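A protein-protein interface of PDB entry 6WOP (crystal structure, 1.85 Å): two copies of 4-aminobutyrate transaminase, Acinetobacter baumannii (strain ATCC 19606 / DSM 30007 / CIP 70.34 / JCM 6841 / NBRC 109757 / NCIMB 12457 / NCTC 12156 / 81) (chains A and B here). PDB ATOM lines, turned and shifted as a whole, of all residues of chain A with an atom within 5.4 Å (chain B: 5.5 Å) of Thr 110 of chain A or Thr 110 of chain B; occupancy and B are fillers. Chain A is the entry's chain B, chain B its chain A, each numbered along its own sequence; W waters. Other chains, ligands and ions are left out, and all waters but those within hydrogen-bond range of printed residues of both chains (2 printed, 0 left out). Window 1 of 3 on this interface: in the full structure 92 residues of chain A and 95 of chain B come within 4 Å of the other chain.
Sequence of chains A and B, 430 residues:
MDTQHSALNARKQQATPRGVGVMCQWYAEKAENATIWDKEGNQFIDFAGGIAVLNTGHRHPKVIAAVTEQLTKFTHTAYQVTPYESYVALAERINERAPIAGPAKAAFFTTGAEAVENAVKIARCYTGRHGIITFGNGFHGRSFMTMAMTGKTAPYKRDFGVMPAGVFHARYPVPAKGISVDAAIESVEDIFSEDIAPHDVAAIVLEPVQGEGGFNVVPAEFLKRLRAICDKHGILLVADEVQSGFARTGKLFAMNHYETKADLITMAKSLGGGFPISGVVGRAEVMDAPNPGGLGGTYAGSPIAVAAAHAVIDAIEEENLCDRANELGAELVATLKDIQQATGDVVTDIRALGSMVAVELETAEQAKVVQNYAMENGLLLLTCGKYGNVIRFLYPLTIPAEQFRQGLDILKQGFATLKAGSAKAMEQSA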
ATOM      1  N   PHE A 108      37.672  24.573 -11.543  1.00  0.00           N
ATOM      2  CA  PHE A 108      36.753  24.094 -10.512  1.00  0.00           C
ATOM      3  C   PHE A 108      35.693  23.198 -11.117  1.00  0.00           C
ATOM      4  O   PHE A 108      35.208  23.465 -12.220  1.00  0.00           O
ATOM      5  CB  PHE A 108      36.104  25.331  -9.802  1.00  0.00           C
ATOM      6  CG  PHE A 108      37.143  26.131  -9.163  1.00  0.00           C
ATOM      7  CD1 PHE A 108      37.841  25.592  -8.090  1.00  0.00           C
ATOM      8  CD2 PHE A 108      37.566  27.356  -9.711  1.00  0.00           C
ATOM      9  CE1 PHE A 108      38.936  26.300  -7.510  1.00  0.00           C
ATOM     10  CE2 PHE A 108      38.670  28.035  -9.153  1.00  0.00           C
ATOM     11  CZ  PHE A 108      39.356  27.504  -8.062  1.00  0.00           C
ATOM     12  N   PHE A 109      35.383  22.114 -10.399  1.00  0.00           N
ATOM     13  CA  PHE A 109      34.291  21.236 -10.747  1.00  0.00           C
ATOM     14  C   PHE A 109      33.329  21.212  -9.569  1.00  0.00           C
ATOM     15  O   PHE A 109      33.264  22.181  -8.763  1.00  0.00           O
ATOM     16  CB  PHE A 109      34.896  19.879 -11.104  1.00  0.00           C
ATOM     17  CG  PHE A 109      35.947  20.016 -12.187  1.00  0.00           C
ATOM     18  CD1 PHE A 109      35.538  20.178 -13.519  1.00  0.00           C
ATOM     19  CD2 PHE A 109      37.322  20.069 -11.873  1.00  0.00           C
ATOM     20  CE1 PHE A 109      36.507  20.370 -14.575  1.00  0.00           C
ATOM     21  CE2 PHE A 109      38.291  20.232 -12.891  1.00  0.00           C
ATOM     22  CZ  PHE A 109      37.835  20.383 -14.251  1.00  0.00           C
ATOM     23  N   THR A 110      32.547  20.152  -9.461  1.00  0.00           N
ATOM     24  CA  THR A 110      31.567  20.101  -8.377  1.00  0.00           C
ATOM     25  C   THR A 110      31.986  19.129  -7.282  1.00  0.00           C
ATOM     26  O   THR A 110      32.043  19.514  -6.117  1.00  0.00           O
ATOM     27  CB  THR A 110      30.180  19.752  -8.965  1.00  0.00           C
ATOM     28  OG1 THR A 110      29.892  20.699 -10.023  1.00  0.00           O
ATOM     29  CG2 THR A 110      29.038  19.956  -7.885  1.00  0.00           C
ATOM     30  N   THR A 111      32.269  17.861  -7.611  1.00  0.00           N
ATOM     31  CA  THR A 111      32.454  16.853  -6.572  1.00  0.00           C
ATOM     32  C   THR A 111      33.929  16.458  -6.441  1.00  0.00           C
ATOM     33  O   THR A 111      34.748  16.719  -7.326  1.00  0.00           O
ATOM     34  CB  THR A 111      31.654  15.571  -6.870  1.00  0.00           C
ATOM     35  OG1 THR A 111      32.231  14.940  -8.039  1.00  0.00           O
ATOM     36  CG2 THR A 111      30.178  15.839  -7.078  1.00  0.00           C
ATOM     37  N   GLY A 112      34.248  15.781  -5.329  1.00  0.00           N
ATOM     38  CA  GLY A 112      35.601  15.274  -5.165  1.00  0.00           C
ATOM     39  C   GLY A 112      35.968  14.264  -6.229  1.00  0.00           C
ATOM     40  O   GLY A 112      37.087  14.272  -6.774  1.00  0.00           O
ATOM     41  N   GLU A 114      34.796  14.138  -9.203  1.00  0.00           N
ATOM     42  CA  GLU A 114      35.069  14.859 -10.458  1.00  0.00           C
ATOM     43  C   GLU A 114      36.475  15.435 -10.465  1.00  0.00           C
ATOM     44  O   GLU A 114      37.150  15.456 -11.504  1.00  0.00           O
ATOM     45  CB  GLU A 114      34.084  16.024 -10.662  1.00  0.00           C
ATOM     46  CG  GLU A 114      33.104  15.806 -11.729  1.00  0.00           C
ATOM     47  CD  GLU A 114      32.067  16.932 -11.771  1.00  0.00           C
ATOM     48  OE1 GLU A 114      31.984  17.695 -10.804  1.00  0.00           O
ATOM     49  OE2 GLU A 114      31.338  17.025 -12.767  1.00  0.00           O
ATOM     50  N   PRO A 276      28.632  22.581  -2.433  1.00  0.00           N
ATOM     51  CA  PRO A 276      29.329  21.680  -3.401  1.00  0.00           C
ATOM     52  C   PRO A 276      30.275  22.388  -4.373  1.00  0.00           C
ATOM     53  O   PRO A 276      29.833  23.211  -5.200  1.00  0.00           O
ATOM     54  CB  PRO A 276      28.185  21.000  -4.159  1.00  0.00           C
ATOM     55  CG  PRO A 276      26.954  21.040  -3.140  1.00  0.00           C
ATOM     56  CD  PRO A 276      27.161  22.455  -2.504  1.00  0.00           C
ATOM     57  N   ILE A 277      31.578  22.119  -4.225  1.00  0.00           N
ATOM     58  CA  ILE A 277      32.572  22.595  -5.189  1.00  0.00           C
ATOM     59  C   ILE A 277      33.823  21.732  -5.052  1.00  0.00           C
ATOM     60  O   ILE A 277      34.085  21.150  -3.985  1.00  0.00           O
ATOM     61  CB  ILE A 277      32.891  24.096  -4.992  1.00  0.00           C
ATOM     62  CG1 ILE A 277      33.912  24.614  -6.073  1.00  0.00           C
ATOM     63  CG2 ILE A 277      33.402  24.289  -3.574  1.00  0.00           C
ATOM     64  CD1 ILE A 277      33.933  26.222  -6.188  1.00  0.00           C
ATOM     65  N   SER A 278      34.580  21.632  -6.139  1.00  0.00           N
ATOM     66  CA  SER A 278      35.849  20.914  -6.104  1.00  0.00           C
ATOM     67  C   SER A 278      36.778  21.591  -7.084  1.00  0.00           C
ATOM     68  O   SER A 278      36.371  22.508  -7.806  1.00  0.00           O
ATOM     69  CB  SER A 278      35.654  19.431  -6.470  1.00  0.00           C
ATOM     70  OG  SER A 278      35.440  19.270  -7.894  1.00  0.00           O
ATOM     71  N   TYR A 299      27.372  22.130 -13.282  1.00  0.00           N
ATOM     72  CA  TYR A 299      27.425  22.742 -11.959  1.00  0.00           C
ATOM     73  C   TYR A 299      28.826  23.185 -11.522  1.00  0.00           C
ATOM     74  O   TYR A 299      28.957  23.794 -10.457  1.00  0.00           O
ATOM     75  CB  TYR A 299      26.952  21.712 -10.923  1.00  0.00           C
ATOM     76  CG  TYR A 299      25.457  21.403 -10.958  1.00  0.00           C
ATOM     77  CD1 TYR A 299      24.498  22.434 -11.104  1.00  0.00           C
ATOM     78  CD2 TYR A 299      25.010  20.133 -10.693  1.00  0.00           C
ATOM     79  CE1 TYR A 299      23.131  22.132 -11.037  1.00  0.00           C
ATOM     80  CE2 TYR A 299      23.632  19.812 -10.696  1.00  0.00           C
ATOM     81  CZ  TYR A 299      22.712  20.824 -10.868  1.00  0.00           C
ATOM     82  OH  TYR A 299      21.341  20.517 -10.830  1.00  0.00           O
ATOM     83  N   ALA A 300      29.851  22.844 -12.276  1.00  0.00           N
ATOM     84  CA  ALA A 300      31.250  23.089 -11.899  1.00  0.00           C
ATOM     85  C   ALA A 300      31.434  24.533 -11.462  1.00  0.00           C
ATOM     86  O   ALA A 300      30.901  25.443 -12.094  1.00  0.00           O
ATOM     87  CB  ALA A 300      32.147  22.823 -13.127  1.00  0.00           C
ATOM     88  N   GLY A 301      32.199  24.759 -10.398  1.00  0.00           N
ATOM     89  CA  GLY A 301      32.449  26.165 -10.044  1.00  0.00           C
ATOM     90  C   GLY A 301      31.207  26.947  -9.682  1.00  0.00           C
ATOM     91  O   GLY A 301      31.072  28.130 -10.067  1.00  0.00           O
ATOM     92  N   PHE B 108      19.261  10.792  -4.257  1.00  0.00           N
ATOM     93  CA  PHE B 108      19.781  12.055  -4.811  1.00  0.00           C
ATOM     94  C   PHE B 108      21.291  12.035  -4.775  1.00  0.00           C
ATOM     95  O   PHE B 108      21.890  11.523  -3.816  1.00  0.00           O
ATOM     96  CB  PHE B 108      19.223  13.273  -4.001  1.00  0.00           C
ATOM     97  CG  PHE B 108      17.739  13.320  -4.088  1.00  0.00           C
ATOM     98  CD1 PHE B 108      17.156  13.601  -5.297  1.00  0.00           C
ATOM     99  CD2 PHE B 108      16.937  12.890  -3.038  1.00  0.00           C
ATOM    100  CE1 PHE B 108      15.791  13.526  -5.468  1.00  0.00           C
ATOM    101  CE2 PHE B 108      15.557  12.827  -3.201  1.00  0.00           C
ATOM    102  CZ  PHE B 108      14.989  13.153  -4.397  1.00  0.00           C
ATOM    103  N   PHE B 109      21.891  12.551  -5.852  1.00  0.00           N
ATOM    104  CA  PHE B 109      23.338  12.731  -5.912  1.00  0.00           C
ATOM    105  C   PHE B 109      23.598  14.205  -6.163  1.00  0.00           C
ATOM    106  O   PHE B 109      22.778  15.043  -5.728  1.00  0.00           O
ATOM    107  CB  PHE B 109      23.887  11.804  -7.006  1.00  0.00           C
ATOM    108  CG  PHE B 109      23.460  10.409  -6.765  1.00  0.00           C
ATOM    109  CD1 PHE B 109      24.097   9.653  -5.767  1.00  0.00           C
ATOM    110  CD2 PHE B 109      22.399   9.860  -7.448  1.00  0.00           C
ATOM    111  CE1 PHE B 109      23.692   8.350  -5.492  1.00  0.00           C
ATOM    112  CE2 PHE B 109      21.978   8.547  -7.149  1.00  0.00           C
ATOM    113  CZ  PHE B 109      22.621   7.837  -6.158  1.00  0.00           C
ATOM    114  N   THR B 110      24.710  14.535  -6.825  1.00  0.00           N
ATOM    115  CA  THR B 110      25.014  15.953  -7.041  1.00  0.00           C
ATOM    116  C   THR B 110      24.950  16.369  -8.498  1.00  0.00           C
ATOM    117  O   THR B 110      24.342  17.403  -8.805  1.00  0.00           O
ATOM    118  CB  THR B 110      26.375  16.313  -6.465  1.00  0.00           C
ATOM    119  OG1 THR B 110      26.449  15.837  -5.106  1.00  0.00           O
ATOM    120  CG2 THR B 110      26.568  17.869  -6.434  1.00  0.00           C
ATOM    121  N   THR B 111      25.591  15.628  -9.408  1.00  0.00           N
ATOM    122  CA  THR B 111      25.656  16.074 -10.798  1.00  0.00           C
ATOM    123  C   THR B 111      24.794  15.229 -11.737  1.00  0.00           C
ATOM    124  O   THR B 111      24.422  14.082 -11.440  1.00  0.00           O
ATOM    125  CB  THR B 111      27.108  16.030 -11.301  1.00  0.00           C
ATOM    126  OG1 THR B 111      27.515  14.657 -11.289  1.00  0.00           O
ATOM    127  CG2 THR B 111      28.073  16.868 -10.396  1.00  0.00           C
ATOM    128  N   GLY B 112      24.529  15.789 -12.921  1.00  0.00           N
ATOM    129  CA  GLY B 112      23.828  15.014 -13.938  1.00  0.00           C
ATOM    130  C   GLY B 112      24.582  13.744 -14.301  1.00  0.00           C
ATOM    131  O   GLY B 112      23.988  12.672 -14.394  1.00  0.00           O
ATOM    132  N   GLU B 114      26.636  12.041 -12.379  1.00  0.00           N
ATOM    133  CA  GLU B 114      26.458  11.099 -11.267  1.00  0.00           C
ATOM    134  C   GLU B 114      25.127  10.403 -11.348  1.00  0.00           C
ATOM    135  O   GLU B 114      25.020   9.218 -11.040  1.00  0.00           O
ATOM    136  CB  GLU B 114      26.550  11.817  -9.902  1.00  0.00           C
ATOM    137  CG  GLU B 114      27.808  11.744  -9.241  1.00  0.00           C
ATOM    138  CD  GLU B 114      27.832  12.568  -7.973  1.00  0.00           C
ATOM    139  OE1 GLU B 114      27.025  13.456  -7.825  1.00  0.00           O
ATOM    140  OE2 GLU B 114      28.677  12.317  -7.129  1.00  0.00           O
ATOM    141  N   PRO B 276      23.284  22.807  -7.039  1.00  0.00           N
ATOM    142  CA  PRO B 276      23.746  21.468  -7.504  1.00  0.00           C
ATOM    143  C   PRO B 276      23.019  20.342  -6.789  1.00  0.00           C
ATOM    144  O   PRO B 276      23.177  20.143  -5.567  1.00  0.00           O
ATOM    145  CB  PRO B 276      25.246  21.464  -7.187  1.00  0.00           C
ATOM    146  CG  PRO B 276      25.642  22.922  -7.259  1.00  0.00           C
ATOM    147  CD  PRO B 276      24.425  23.650  -6.633  1.00  0.00           C
ATOM    148  N   ILE B 277      22.272  19.561  -7.581  1.00  0.00           N
ATOM    149  CA  ILE B 277      21.665  18.318  -7.119  1.00  0.00           C
ATOM    150  C   ILE B 277      21.259  17.529  -8.352  1.00  0.00           C
ATOM    151  O   ILE B 277      20.958  18.110  -9.401  1.00  0.00           O
ATOM    152  CB  ILE B 277      20.435  18.615  -6.216  1.00  0.00           C
ATOM    153  CG1 ILE B 277      19.775  17.326  -5.697  1.00  0.00           C
ATOM    154  CG2 ILE B 277      19.378  19.454  -6.980  1.00  0.00           C
ATOM    155  CD1 ILE B 277      18.751  17.535  -4.489  1.00  0.00           C
ATOM    156  N   SER B 278      21.132  16.202  -8.193  1.00  0.00           N
ATOM    157  CA  SER B 278      20.692  15.268  -9.245  1.00  0.00           C
ATOM    158  C   SER B 278      19.914  14.160  -8.567  1.00  0.00           C
ATOM    159  O   SER B 278      19.802  14.134  -7.333  1.00  0.00           O
ATOM    160  CB  SER B 278      21.873  14.654 -10.007  1.00  0.00           C
ATOM    161  OG  SER B 278      22.591  13.771  -9.152  1.00  0.00           O
ATOM    162  N   TYR B 299      28.634  15.209  -1.283  1.00  0.00           N
ATOM    163  CA  TYR B 299      27.714  16.313  -1.547  1.00  0.00           C
ATOM    164  C   TYR B 299      26.323  15.861  -1.965  1.00  0.00           C
ATOM    165  O   TYR B 299      25.463  16.709  -2.219  1.00  0.00           O
ATOM    166  CB  TYR B 299      28.256  17.214  -2.652  1.00  0.00           C
ATOM    167  CG  TYR B 299      29.504  18.029  -2.302  1.00  0.00           C
ATOM    168  CD1 TYR B 299      29.636  18.694  -1.045  1.00  0.00           C
ATOM    169  CD2 TYR B 299      30.484  18.207  -3.255  1.00  0.00           C
ATOM    170  CE1 TYR B 299      30.822  19.478  -0.773  1.00  0.00           C
ATOM    171  CE2 TYR B 299      31.675  18.950  -3.001  1.00  0.00           C
ATOM    172  CZ  TYR B 299      31.831  19.557  -1.778  1.00  0.00           C
ATOM    173  OH  TYR B 299      32.994  20.282  -1.604  1.00  0.00           O
ATOM    174  N   ALA B 300      26.077  14.571  -2.092  1.00  0.00           N
ATOM    175  CA  ALA B 300      24.818  14.093  -2.627  1.00  0.00           C
ATOM    176  C   ALA B 300      23.614  14.661  -1.846  1.00  0.00           C
ATOM    177  O   ALA B 300      23.608  14.640  -0.618  1.00  0.00           O
ATOM    178  CB  ALA B 300      24.789  12.556  -2.520  1.00  0.00           C
ATOM    179  N   GLY B 301      22.579  15.116  -2.565  1.00  0.00           N
ATOM    180  CA  GLY B 301      21.343  15.549  -1.907  1.00  0.00           C
ATOM    181  C   GLY B 301      21.603  16.709  -0.969  1.00  0.00           C
ATOM    182  O   GLY B 301      21.146  16.711   0.171  1.00  0.00           O
HETATM  183  O   HOH W   1      29.884  14.008 -11.879  1.00  0.00           O
HETATM  184  O   HOH W   2      31.091  12.976  -9.304  1.00  0.00           O
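Water W1 lies within hydrogen-bond range of OG1 of Thr 111 of chain B and OE2 of Glu 114 of chain A.
Water W2 bridges OG1 of Thr 111 of chain A (2.6 Å) and OE2 of Glu 114 of chain B (3.3 Å).
Of the 12 printed residues of chain B, 6 touch a printed residue of chain A.
Printed residues of chain B that touch a printed residue of chain A: Thr 110, Thr 111, Glu 114, Pro 276, Ile 277 and Tyr 299.
Hydrophobic or aromatic side chains of chain B that line the printed part of chain A: Pro 276 and Tyr 299.
Among the printed residues, 10 pairs touch across the chains.
Among the printed residues, no Asp or Glu carboxylate lies within 4 Å of a Lys or Arg side-chain nitrogen of the other chain.
Thr 110 of chain A touches its own counterpart, Thr 110 of chain B.
Thr 110 of chain A touches Thr 111 of chain B, and with the chains exchanged Thr 111 of chain A touches Thr 110 of chain B.
Thr 111 of chain A touches Glu 114 of chain B, but with the chains exchanged Glu 114 of chain A does not touch Thr 111 of chain B (4.02 Å).
Ile 277 of chain A touches Tyr 299 of chain B, and with the chains exchanged Tyr 299 of chain A touches Ile 277 of chain B.
Of the 10 pairs that touch across the chains among the printed residues, 9 have their exchanged pair printed and touching as well.
Thr 110 of chain A touches just these residues of chain B: Thr 110 (3.5 Å), Thr 111 (3.8 Å) and Tyr 299 (3.2 Å).
Of the printed residues of chain B, Thr 111 of chain A touches Thr 110 and Glu 114.
Of the printed residues of chain B, Tyr 299 of chain A touches Thr 110, Pro 276 and Ile 277.
Of chain A, only Thr 110 (3.5 Å), Thr 111 (3.9 Å) and Tyr 299 (3.1 Å) come within 4 Å of Thr 110 of chain B.
Printed residues of chain A within 4 Å of Thr 111 of chain B: Thr 110 (3.8 Å).
Gly 112 of chain B touches none of the printed residues of chain A.
The nearest residue of chain B that does not touch Thr 110 of chain A is Pro 276 of chain B (4.1 Å).
The nearest printed residue of chain A that does not touch Thr 111 of chain B is Glu 114 of chain A (4.02 Å).
Among the printed residues, pairs that only touch across the chains: Thr 110 of chain A with Thr 110 of chain B (3.5 Å), Thr 110 of chain A with Thr 111 of chain B (3.8 Å), Thr 110 of chain A with Tyr 299 of chain B (3.2 Å), Thr 111 of chain A with Thr 110 of chain B (3.9 Å), Thr 111 of chain A with Glu 114 of chain B (3.8 Å), Pro 276 of chain A with Tyr 299 of chain B (3.6 Å), Tyr 299 of chain A with Thr 110 of chain B (3.1 Å) and Tyr 299 of chain A with Pro 276 of chain B (3.6 Å).
The side-chain carboxylate (OE1) of Glu 114 of chain B lies within hydrogen-bond range of the backbone NH (N) of Thr 110 of chain B (2.7 Å).
OG1 of Thr 111 of chain A is in hydrogen-bond range of N of Glu 114 of chain A (2.9 Å).
OE1 of Glu 114 of chain A lies within hydrogen-bond range of N of Thr 110 of chain A (2.9 Å).
O of Thr 111 of chain B is in hydrogen-bond range of OG of Ser 278 of chain B (2.9 Å).
The backbone NH (N) of Ala 300 of chain B sits at hydrogen-bond distance from the side-chain hydroxyl (OG1) of Thr 110 of chain B (3.3 Å).
The backbone NH (N) of Ala 300 of chain A is in hydrogen-bond range of the side-chain hydroxyl (OG1) of Thr 110 of chain A (3.1 Å).
The backbone carbonyl oxygen (O) of Ile 277 of chain B lies within hydrogen-bond range of the side-chain hydroxyl (OH) of Tyr 299 of chain A.
OH of Tyr 299 of chain B sits at hydrogen-bond distance from O of Ile 277 of chain A (2.8 Å).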
